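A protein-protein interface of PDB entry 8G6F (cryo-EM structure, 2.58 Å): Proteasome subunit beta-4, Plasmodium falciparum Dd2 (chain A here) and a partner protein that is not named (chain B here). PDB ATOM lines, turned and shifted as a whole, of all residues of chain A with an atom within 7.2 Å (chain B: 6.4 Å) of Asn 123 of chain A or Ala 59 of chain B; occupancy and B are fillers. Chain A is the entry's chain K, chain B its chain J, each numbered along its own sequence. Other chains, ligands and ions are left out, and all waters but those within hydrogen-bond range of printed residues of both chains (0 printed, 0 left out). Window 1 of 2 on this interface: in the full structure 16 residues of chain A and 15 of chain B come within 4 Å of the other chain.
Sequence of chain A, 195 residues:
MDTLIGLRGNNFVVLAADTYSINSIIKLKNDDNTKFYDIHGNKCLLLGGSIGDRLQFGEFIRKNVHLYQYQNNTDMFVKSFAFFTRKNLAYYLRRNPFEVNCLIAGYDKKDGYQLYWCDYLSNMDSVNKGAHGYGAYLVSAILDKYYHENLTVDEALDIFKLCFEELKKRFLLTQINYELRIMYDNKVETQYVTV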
ATOM      1  N   ARG A  86      20.188 -16.194  29.750  1.00  0.00           N
ATOM      2  CA  ARG A  86      19.122 -16.883  29.036  1.00  0.00           C
ATOM      3  C   ARG A  86      19.558 -18.278  28.614  1.00  0.00           C
ATOM      4  O   ARG A  86      18.776 -19.228  28.691  1.00  0.00           O
ATOM      5  CB  ARG A  86      18.691 -16.063  27.822  1.00  0.00           C
ATOM      6  CG  ARG A  86      17.435 -16.567  27.145  1.00  0.00           C
ATOM      7  CD  ARG A  86      17.546 -16.476  25.641  1.00  0.00           C
ATOM      8  NE  ARG A  86      18.398 -17.525  25.093  1.00  0.00           N
ATOM      9  CZ  ARG A  86      17.972 -18.719  24.704  1.00  0.00           C
ATOM     10  NH1 ARG A  86      16.698 -19.058  24.773  1.00  0.00           N
ATOM     11  NH2 ARG A  86      18.849 -19.597  24.234  1.00  0.00           N
ATOM     12  N   LEU A  89      19.472 -20.554  31.692  1.00  0.00           N
ATOM     13  CA  LEU A  89      18.097 -20.871  32.051  1.00  0.00           C
ATOM     14  C   LEU A  89      17.490 -21.866  31.070  1.00  0.00           C
ATOM     15  O   LEU A  89      16.811 -22.814  31.475  1.00  0.00           O
ATOM     16  CB  LEU A  89      17.271 -19.588  32.105  1.00  0.00           C
ATOM     17  CG  LEU A  89      15.997 -19.582  32.943  1.00  0.00           C
ATOM     18  CD1 LEU A  89      16.273 -19.990  34.373  1.00  0.00           C
ATOM     19  CD2 LEU A  89      15.372 -18.213  32.898  1.00  0.00           C
ATOM     20  N   CYS A 102      13.249 -13.037  35.144  1.00  0.00           N
ATOM     21  CA  CYS A 102      14.444 -12.210  35.179  1.00  0.00           C
ATOM     22  C   CYS A 102      14.196 -10.867  34.508  1.00  0.00           C
ATOM     23  O   CYS A 102      13.564 -10.786  33.451  1.00  0.00           O
ATOM     24  CB  CYS A 102      15.616 -12.910  34.483  1.00  0.00           C
ATOM     25  SG  CYS A 102      15.600 -14.707  34.603  1.00  0.00           S
ATOM     26  N   TRP A 117      13.959  -8.539  29.311  1.00  0.00           N
ATOM     27  CA  TRP A 117      12.853  -9.210  29.977  1.00  0.00           C
ATOM     28  C   TRP A 117      12.950 -10.695  29.664  1.00  0.00           C
ATOM     29  O   TRP A 117      13.072 -11.068  28.497  1.00  0.00           O
ATOM     30  CB  TRP A 117      11.529  -8.623  29.480  1.00  0.00           C
ATOM     31  CG  TRP A 117      10.266  -9.208  30.044  1.00  0.00           C
ATOM     32  CD1 TRP A 117       9.497  -8.679  31.031  1.00  0.00           C
ATOM     33  CD2 TRP A 117       9.607 -10.405  29.623  1.00  0.00           C
ATOM     34  NE1 TRP A 117       8.410  -9.474  31.262  1.00  0.00           N
ATOM     35  CE2 TRP A 117       8.455 -10.544  30.411  1.00  0.00           C
ATOM     36  CE3 TRP A 117       9.887 -11.380  28.663  1.00  0.00           C
ATOM     37  CZ2 TRP A 117       7.583 -11.615  30.272  1.00  0.00           C
ATOM     38  CZ3 TRP A 117       9.024 -12.440  28.529  1.00  0.00           C
ATOM     39  CH2 TRP A 117       7.883 -12.548  29.325  1.00  0.00           C
ATOM     40  N   CYS A 118      12.914 -11.539  30.694  1.00  0.00           N
ATOM     41  CA  CYS A 118      13.027 -12.980  30.509  1.00  0.00           C
ATOM     42  C   CYS A 118      12.047 -13.672  31.440  1.00  0.00           C
ATOM     43  O   CYS A 118      11.950 -13.303  32.610  1.00  0.00           O
ATOM     44  CB  CYS A 118      14.456 -13.456  30.794  1.00  0.00           C
ATOM     45  SG  CYS A 118      14.890 -15.061  30.101  1.00  0.00           S
ATOM     46  N   ASP A 119      11.324 -14.664  30.938  1.00  0.00           N
ATOM     47  CA  ASP A 119      10.376 -15.398  31.762  1.00  0.00           C
ATOM     48  C   ASP A 119      10.940 -16.766  32.123  1.00  0.00           C
ATOM     49  O   ASP A 119      12.012 -17.169  31.667  1.00  0.00           O
ATOM     50  CB  ASP A 119       9.021 -15.528  31.059  1.00  0.00           C
ATOM     51  CG  ASP A 119       9.090 -16.338  29.791  1.00  0.00           C
ATOM     52  OD1 ASP A 119      10.191 -16.786  29.427  1.00  0.00           O
ATOM     53  OD2 ASP A 119       8.037 -16.529  29.155  1.00  0.00           O
ATOM     54  N   TYR A 120      10.199 -17.481  32.971  1.00  0.00           N
ATOM     55  CA  TYR A 120      10.667 -18.771  33.463  1.00  0.00           C
ATOM     56  C   TYR A 120      10.847 -19.783  32.343  1.00  0.00           C
ATOM     57  O   TYR A 120      11.559 -20.774  32.529  1.00  0.00           O
ATOM     58  CB  TYR A 120       9.693 -19.317  34.503  1.00  0.00           C
ATOM     59  CG  TYR A 120       8.374 -19.749  33.920  1.00  0.00           C
ATOM     60  CD1 TYR A 120       7.410 -18.818  33.579  1.00  0.00           C
ATOM     61  CD2 TYR A 120       8.094 -21.088  33.708  1.00  0.00           C
ATOM     62  CE1 TYR A 120       6.208 -19.206  33.045  1.00  0.00           C
ATOM     63  CE2 TYR A 120       6.895 -21.484  33.175  1.00  0.00           C
ATOM     64  CZ  TYR A 120       5.955 -20.539  32.845  1.00  0.00           C
ATOM     65  OH  TYR A 120       4.752 -20.930  32.313  1.00  0.00           O
ATOM     66  N   LEU A 121      10.220 -19.563  31.191  1.00  0.00           N
ATOM     67  CA  LEU A 121      10.441 -20.407  30.027  1.00  0.00           C
ATOM     68  C   LEU A 121      11.673 -19.999  29.240  1.00  0.00           C
ATOM     69  O   LEU A 121      11.992 -20.654  28.245  1.00  0.00           O
ATOM     70  CB  LEU A 121       9.219 -20.372  29.111  1.00  0.00           C
ATOM     71  CG  LEU A 121       7.967 -21.093  29.606  1.00  0.00           C
ATOM     72  CD1 LEU A 121       6.872 -20.988  28.574  1.00  0.00           C
ATOM     73  CD2 LEU A 121       8.261 -22.548  29.928  1.00  0.00           C
ATOM     74  N   SER A 122      12.364 -18.940  29.661  1.00  0.00           N
ATOM     75  CA  SER A 122      13.577 -18.471  29.006  1.00  0.00           C
ATOM     76  C   SER A 122      13.273 -17.753  27.696  1.00  0.00           C
ATOM     77  O   SER A 122      14.099 -17.746  26.781  1.00  0.00           O
ATOM     78  CB  SER A 122      14.528 -19.641  28.765  1.00  0.00           C
ATOM     79  OG  SER A 122      15.873 -19.217  28.839  1.00  0.00           O
ATOM     80  N   ASN A 123      12.102 -17.134  27.604  1.00  0.00           N
ATOM     81  CA  ASN A 123      11.750 -16.282  26.473  1.00  0.00           C
ATOM     82  C   ASN A 123      12.239 -14.871  26.776  1.00  0.00           C
ATOM     83  O   ASN A 123      11.684 -14.191  27.641  1.00  0.00           O
ATOM     84  CB  ASN A 123      10.243 -16.295  26.231  1.00  0.00           C
ATOM     85  CG  ASN A 123       9.698 -17.686  26.008  1.00  0.00           C
ATOM     86  OD1 ASN A 123      10.247 -18.463  25.238  1.00  0.00           O
ATOM     87  ND2 ASN A 123       8.609 -18.008  26.686  1.00  0.00           N
ATOM     88  N   MET A 124      13.267 -14.425  26.060  1.00  0.00           N
ATOM     89  CA  MET A 124      13.924 -13.160  26.352  1.00  0.00           C
ATOM     90  C   MET A 124      13.813 -12.202  25.176  1.00  0.00           C
ATOM     91  O   MET A 124      13.726 -12.616  24.019  1.00  0.00           O
ATOM     92  CB  MET A 124      15.399 -13.365  26.692  1.00  0.00           C
ATOM     93  CG  MET A 124      15.998 -12.220  27.485  1.00  0.00           C
ATOM     94  SD  MET A 124      17.765 -12.368  27.773  1.00  0.00           S
ATOM     95  CE  MET A 124      18.384 -12.420  26.098  1.00  0.00           C
ATOM     96  N   ASP A 125      13.817 -10.911  25.493  1.00  0.00           N
ATOM     97  CA  ASP A 125      13.891  -9.856  24.494  1.00  0.00           C
ATOM     98  C   ASP A 125      14.193  -8.544  25.198  1.00  0.00           C
ATOM     99  O   ASP A 125      13.741  -8.317  26.320  1.00  0.00           O
ATOM    100  CB  ASP A 125      12.592  -9.742  23.690  1.00  0.00           C
ATOM    101  CG  ASP A 125      12.758  -8.908  22.436  1.00  0.00           C
ATOM    102  OD1 ASP A 125      13.791  -9.062  21.751  1.00  0.00           O
ATOM    103  OD2 ASP A 125      11.862  -8.098  22.133  1.00  0.00           O
ATOM    104  N   HIS A 132       7.029  -8.294  35.733  1.00  0.00           N
ATOM    105  CA  HIS A 132       6.813  -9.697  36.045  1.00  0.00           C
ATOM    106  C   HIS A 132       5.945  -9.804  37.286  1.00  0.00           C
ATOM    107  O   HIS A 132       5.951  -8.920  38.145  1.00  0.00           O
ATOM    108  CB  HIS A 132       8.131 -10.436  36.279  1.00  0.00           C
ATOM    109  CG  HIS A 132       8.819 -10.860  35.021  1.00  0.00           C
ATOM    110  ND1 HIS A 132      10.080 -10.424  34.684  1.00  0.00           N
ATOM    111  CD2 HIS A 132       8.427 -11.687  34.025  1.00  0.00           C
ATOM    112  CE1 HIS A 132      10.433 -10.960  33.531  1.00  0.00           C
ATOM    113  NE2 HIS A 132       9.449 -11.731  33.112  1.00  0.00           N
ATOM    114  N   TYR B   7       1.330 -20.184  23.373  1.00  0.00           N
ATOM    115  CA  TYR B   7       1.902 -19.414  24.474  1.00  0.00           C
ATOM    116  C   TYR B   7       2.477 -18.091  23.986  1.00  0.00           C
ATOM    117  O   TYR B   7       2.263 -17.048  24.611  1.00  0.00           O
ATOM    118  CB  TYR B   7       2.979 -20.225  25.191  1.00  0.00           C
ATOM    119  CG  TYR B   7       3.570 -19.504  26.382  1.00  0.00           C
ATOM    120  CD1 TYR B   7       4.619 -18.616  26.226  1.00  0.00           C
ATOM    121  CD2 TYR B   7       3.068 -19.702  27.656  1.00  0.00           C
ATOM    122  CE1 TYR B   7       5.154 -17.950  27.300  1.00  0.00           C
ATOM    123  CE2 TYR B   7       3.599 -19.042  28.741  1.00  0.00           C
ATOM    124  CZ  TYR B   7       4.640 -18.167  28.557  1.00  0.00           C
ATOM    125  OH  TYR B   7       5.179 -17.502  29.632  1.00  0.00           O
ATOM    126  N   ASN B   8       3.214 -18.110  22.878  1.00  0.00           N
ATOM    127  CA  ASN B   8       3.814 -16.906  22.313  1.00  0.00           C
ATOM    128  C   ASN B   8       3.110 -16.410  21.063  1.00  0.00           C
ATOM    129  O   ASN B   8       2.998 -15.199  20.871  1.00  0.00           O
ATOM    130  CB  ASN B   8       5.289 -17.154  21.973  1.00  0.00           C
ATOM    131  CG  ASN B   8       6.175 -17.207  23.196  1.00  0.00           C
ATOM    132  OD1 ASN B   8       6.951 -18.141  23.362  1.00  0.00           O
ATOM    133  ND2 ASN B   8       6.076 -16.203  24.050  1.00  0.00           N
ATOM    134  N   LEU B  29       5.955 -10.407  20.681  1.00  0.00           N
ATOM    135  CA  LEU B  29       6.343 -11.441  21.633  1.00  0.00           C
ATOM    136  C   LEU B  29       5.268 -11.513  22.704  1.00  0.00           C
ATOM    137  O   LEU B  29       4.953 -10.504  23.340  1.00  0.00           O
ATOM    138  CB  LEU B  29       7.708 -11.155  22.260  1.00  0.00           C
ATOM    139  CG  LEU B  29       8.170 -12.204  23.275  1.00  0.00           C
ATOM    140  CD1 LEU B  29       8.273 -13.577  22.631  1.00  0.00           C
ATOM    141  CD2 LEU B  29       9.486 -11.813  23.908  1.00  0.00           C
ATOM    142  N   GLY B  30       4.708 -12.705  22.904  1.00  0.00           N
ATOM    143  CA  GLY B  30       3.602 -12.900  23.810  1.00  0.00           C
ATOM    144  C   GLY B  30       4.005 -13.638  25.075  1.00  0.00           C
ATOM    145  O   GLY B  30       5.125 -14.114  25.234  1.00  0.00           O
ATOM    146  N   PHE B  41      10.079  -8.190  18.399  1.00  0.00           N
ATOM    147  CA  PHE B  41      10.701  -9.511  18.433  1.00  0.00           C
ATOM    148  C   PHE B  41      10.691 -10.070  17.018  1.00  0.00           C
ATOM    149  O   PHE B  41       9.742 -10.723  16.588  1.00  0.00           O
ATOM    150  CB  PHE B  41       9.970 -10.420  19.407  1.00  0.00           C
ATOM    151  CG  PHE B  41      10.624 -11.751  19.600  1.00  0.00           C
ATOM    152  CD1 PHE B  41      11.795 -11.862  20.319  1.00  0.00           C
ATOM    153  CD2 PHE B  41      10.062 -12.892  19.068  1.00  0.00           C
ATOM    154  CE1 PHE B  41      12.394 -13.085  20.498  1.00  0.00           C
ATOM    155  CE2 PHE B  41      10.659 -14.117  19.242  1.00  0.00           C
ATOM    156  CZ  PHE B  41      11.825 -14.214  19.958  1.00  0.00           C
ATOM    157  N   GLY B  57       7.252 -19.889  16.788  1.00  0.00           N
ATOM    158  CA  GLY B  57       6.996 -20.867  17.824  1.00  0.00           C
ATOM    159  C   GLY B  57       7.410 -20.363  19.185  1.00  0.00           C
ATOM    160  O   GLY B  57       7.354 -19.160  19.445  1.00  0.00           O
ATOM    161  N   LEU B  58       7.823 -21.270  20.064  1.00  0.00           N
ATOM    162  CA  LEU B  58       8.302 -20.872  21.378  1.00  0.00           C
ATOM    163  C   LEU B  58       9.549 -20.013  21.236  1.00  0.00           C
ATOM    164  O   LEU B  58      10.478 -20.372  20.514  1.00  0.00           O
ATOM    165  CB  LEU B  58       8.596 -22.114  22.215  1.00  0.00           C
ATOM    166  CG  LEU B  58       8.664 -21.938  23.729  1.00  0.00           C
ATOM    167  CD1 LEU B  58       7.336 -21.479  24.299  1.00  0.00           C
ATOM    168  CD2 LEU B  58       9.105 -23.235  24.365  1.00  0.00           C
ATOM    169  N   ALA B  59       9.566 -18.873  21.929  1.00  0.00           N
ATOM    170  CA  ALA B  59      10.638 -17.902  21.732  1.00  0.00           C
ATOM    171  C   ALA B  59      11.988 -18.458  22.166  1.00  0.00           C
ATOM    172  O   ALA B  59      13.009 -18.218  21.506  1.00  0.00           O
ATOM    173  CB  ALA B  59      10.320 -16.617  22.491  1.00  0.00           C
ATOM    174  N   THR B  60      12.021 -19.185  23.282  1.00  0.00           N
ATOM    175  CA  THR B  60      13.278 -19.768  23.735  1.00  0.00           C
ATOM    176  C   THR B  60      13.810 -20.770  22.719  1.00  0.00           C
ATOM    177  O   THR B  60      15.013 -20.803  22.439  1.00  0.00           O
ATOM    178  CB  THR B  60      13.101 -20.421  25.108  1.00  0.00           C
ATOM    179  OG1 THR B  60      14.290 -21.137  25.461  1.00  0.00           O
ATOM    180  CG2 THR B  60      11.916 -21.370  25.133  1.00  0.00           C
ATOM    181  N   ASP B  61      12.925 -21.587  22.143  1.00  0.00           N
ATOM    182  CA  ASP B  61      13.356 -22.531  21.121  1.00  0.00           C
ATOM    183  C   ASP B  61      13.801 -21.814  19.858  1.00  0.00           C
ATOM    184  O   ASP B  61      14.732 -22.266  19.191  1.00  0.00           O
ATOM    185  CB  ASP B  61      12.233 -23.514  20.800  1.00  0.00           C
ATOM    186  CG  ASP B  61      12.174 -24.669  21.773  1.00  0.00           C
ATOM    187  OD1 ASP B  61      13.235 -25.080  22.283  1.00  0.00           O
ATOM    188  OD2 ASP B  61      11.066 -25.180  22.022  1.00  0.00           O
ATOM    189  N   ILE B  62      13.157 -20.699  19.516  1.00  0.00           N
ATOM    190  CA  ILE B  62      13.587 -19.916  18.362  1.00  0.00           C
ATOM    191  C   ILE B  62      15.014 -19.435  18.562  1.00  0.00           C
ATOM    192  O   ILE B  62      15.867 -19.576  17.681  1.00  0.00           O
ATOM    193  CB  ILE B  62      12.629 -18.734  18.131  1.00  0.00           C
ATOM    194  CG1 ILE B  62      11.272 -19.231  17.647  1.00  0.00           C
ATOM    195  CG2 ILE B  62      13.219 -17.760  17.130  1.00  0.00           C
ATOM    196  CD1 ILE B  62      10.187 -18.206  17.774  1.00  0.00           C
ATOM    197  N   GLN B  63      15.292 -18.857  19.732  1.00  0.00           N
ATOM    198  CA  GLN B  63      16.630 -18.337  19.994  1.00  0.00           C
ATOM    199  C   GLN B  63      17.662 -19.459  20.019  1.00  0.00           C
ATOM    200  O   GLN B  63      18.754 -19.321  19.456  1.00  0.00           O
ATOM    201  CB  GLN B  63      16.634 -17.560  21.309  1.00  0.00           C
ATOM    202  CG  GLN B  63      17.947 -16.873  21.645  1.00  0.00           C
ATOM    203  CD  GLN B  63      18.420 -15.936  20.557  1.00  0.00           C
ATOM    204  OE1 GLN B  63      17.620 -15.289  19.888  1.00  0.00           O
ATOM    205  NE2 GLN B  63      19.730 -15.864  20.369  1.00  0.00           N
ATOM    206  N   THR B  64      17.327 -20.583  20.653  1.00  0.00           N
ATOM    207  CA  THR B  64      18.252 -21.710  20.707  1.00  0.00           C
ATOM    208  C   THR B  64      18.554 -22.246  19.314  1.00  0.00           C
ATOM    209  O   THR B  64      19.717 -22.482  18.963  1.00  0.00           O
ATOM    210  CB  THR B  64      17.663 -22.814  21.584  1.00  0.00           C
ATOM    211  OG1 THR B  64      17.474 -22.322  22.912  1.00  0.00           O
ATOM    212  CG2 THR B  64      18.581 -24.017  21.619  1.00  0.00           C
ATOM    213  N   PHE B 106      10.136 -26.635  19.759  1.00  0.00           N
ATOM    214  CA  PHE B 106       8.792 -26.227  19.360  1.00  0.00           C
ATOM    215  C   PHE B 106       8.887 -24.996  18.463  1.00  0.00           C
ATOM    216  O   PHE B 106       8.515 -23.879  18.818  1.00  0.00           O
ATOM    217  CB  PHE B 106       7.930 -25.990  20.588  1.00  0.00           C
ATOM    218  CG  PHE B 106       7.706 -27.227  21.391  1.00  0.00           C
ATOM    219  CD1 PHE B 106       7.055 -28.312  20.838  1.00  0.00           C
ATOM    220  CD2 PHE B 106       8.168 -27.322  22.685  1.00  0.00           C
ATOM    221  CE1 PHE B 106       6.857 -29.456  21.563  1.00  0.00           C
ATOM    222  CE2 PHE B 106       7.972 -28.467  23.414  1.00  0.00           C
ATOM    223  CZ  PHE B 106       7.316 -29.537  22.852  1.00  0.00           C
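OD2 of Asp 119 of chain A is in hydrogen-bond range of OH of Tyr 7 of chain B (3.1 Å).
The side-chain amide oxygen of Asn 123 of chain A sits close to the backbone NH of Ala 59 of chain B (3.4 Å).
The guanidinium group (NH1) of Arg 86 of chain A is in hydrogen-bond range of the side-chain hydroxyl (OG1) of Thr 60 of chain B (3.3 Å).
N of Thr 60 of chain B sits at hydrogen-bond distance from OD1 of Asn 123 of chain A (2.7 Å).
The side-chain hydroxyl of Thr 64 of chain B lies within hydrogen-bond range of the guanidinium group of Arg 86 of chain A (3.3 Å).
The backbone carbonyl oxygen (O) of Gly 30 of chain B is in hydrogen-bond range of the side-chain amide nitrogen (ND2) of Asn 8 of chain B, 2.6 Å away.
The backbone NH (N) of Ala 59 of chain B lies within hydrogen-bond range of the side-chain amide oxygen (OD1) of Asn 8 of chain B, 3.1 Å away.
OG of Ser 122 of chain A sits at hydrogen-bond distance from O of Arg 86 of chain A, 2.9 Å away.
N of Trp 117 of chain A sits at hydrogen-bond distance from O of Asp 125 of chain A (3.0 Å).
The side-chain carboxylate (OD1) of Asp 119 of chain A lies close to the backbone NH (N) of Leu 121 of chain A, 3.3 Å away.
N of Ser 122 of chain A lies within hydrogen-bond range of OD1 of Asp 119 of chain A (3.1 Å).
Arg 86 of chain A touches Gln 63 of chain B (NE to CG, 3.5 Å).
Tyr 120 of chain A touches Tyr 7 of chain B (CE1 to OH, 3.95 Å).
Tyr 7 of chain B touches Leu 121 of chain A.
Leu 121 of chain A touches Thr 60 of chain B.
Thr 60 of chain B touches Ser 122 of chain A (CB to O, 3.3 Å).
Asn 123 of chain A touches Tyr 7 of chain B (ND2 to CE1, 3.5 Å).
ND2 of Asn 123 of chain A touches OD1 of Asn 8 of chain B, 3.7 Å away.
O of Met 124 of chain A touches CE1 of Phe 41 of chain B, 3.8 Å away.
Asp 125 of chain A touches Leu 29 of chain B.
Asp 125 of chain A touches Phe 41 of chain B (OD1 to CD1, 3.7 Å).
Printed residues of chain B within 4 Å of Asn 123 of chain A: Tyr 7, Asn 8, Ala 59 and Thr 60.
Of chain A, only Asn 123 (3.3 Å) comes within 4 Å of Ala 59 of chain B.
Printed residues of chain B within 4 Å of Leu 121 of chain A: Tyr 7 (3.6 Å) and Thr 60 (3.2 Å).
Of the printed residues of chain A, Phe 41 of chain B touches Met 124 and Asp 125.
Of the printed residues of chain A, Asn 8 of chain B touches Asn 123.
The nearest residue of chain B that does not touch Asn 123 of chain A is Leu 58 of chain B (4.1 Å).
The nearest residue of chain A that does not touch Ala 59 of chain B is Arg 86 of chain A (5.0 Å).
The nearest printed residue of chain B that does not touch Arg 86 of chain A is Ala 59 of chain B (5.0 Å).
Printed residues of chain B that touch a printed residue of chain A: Tyr 7, Asn 8, Leu 29, Phe 41, Ala 59, Thr 60, Gln 63 and Thr 64.
Printed residues of chain A that touch a printed residue of chain B: Arg 86, Asp 119, Tyr 120, Leu 121, Ser 122, Asn 123, Met 124 and Asp 125.
Along chain A the printed residues that touch a printed residue of chain B span positions 86 to 125.
Among the printed residues, 15 pairs touch across the chains.
Among the printed residues, no Asp or Glu carboxylate lies within 4 Å of a Lys or Arg side-chain nitrogen of the other chain.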
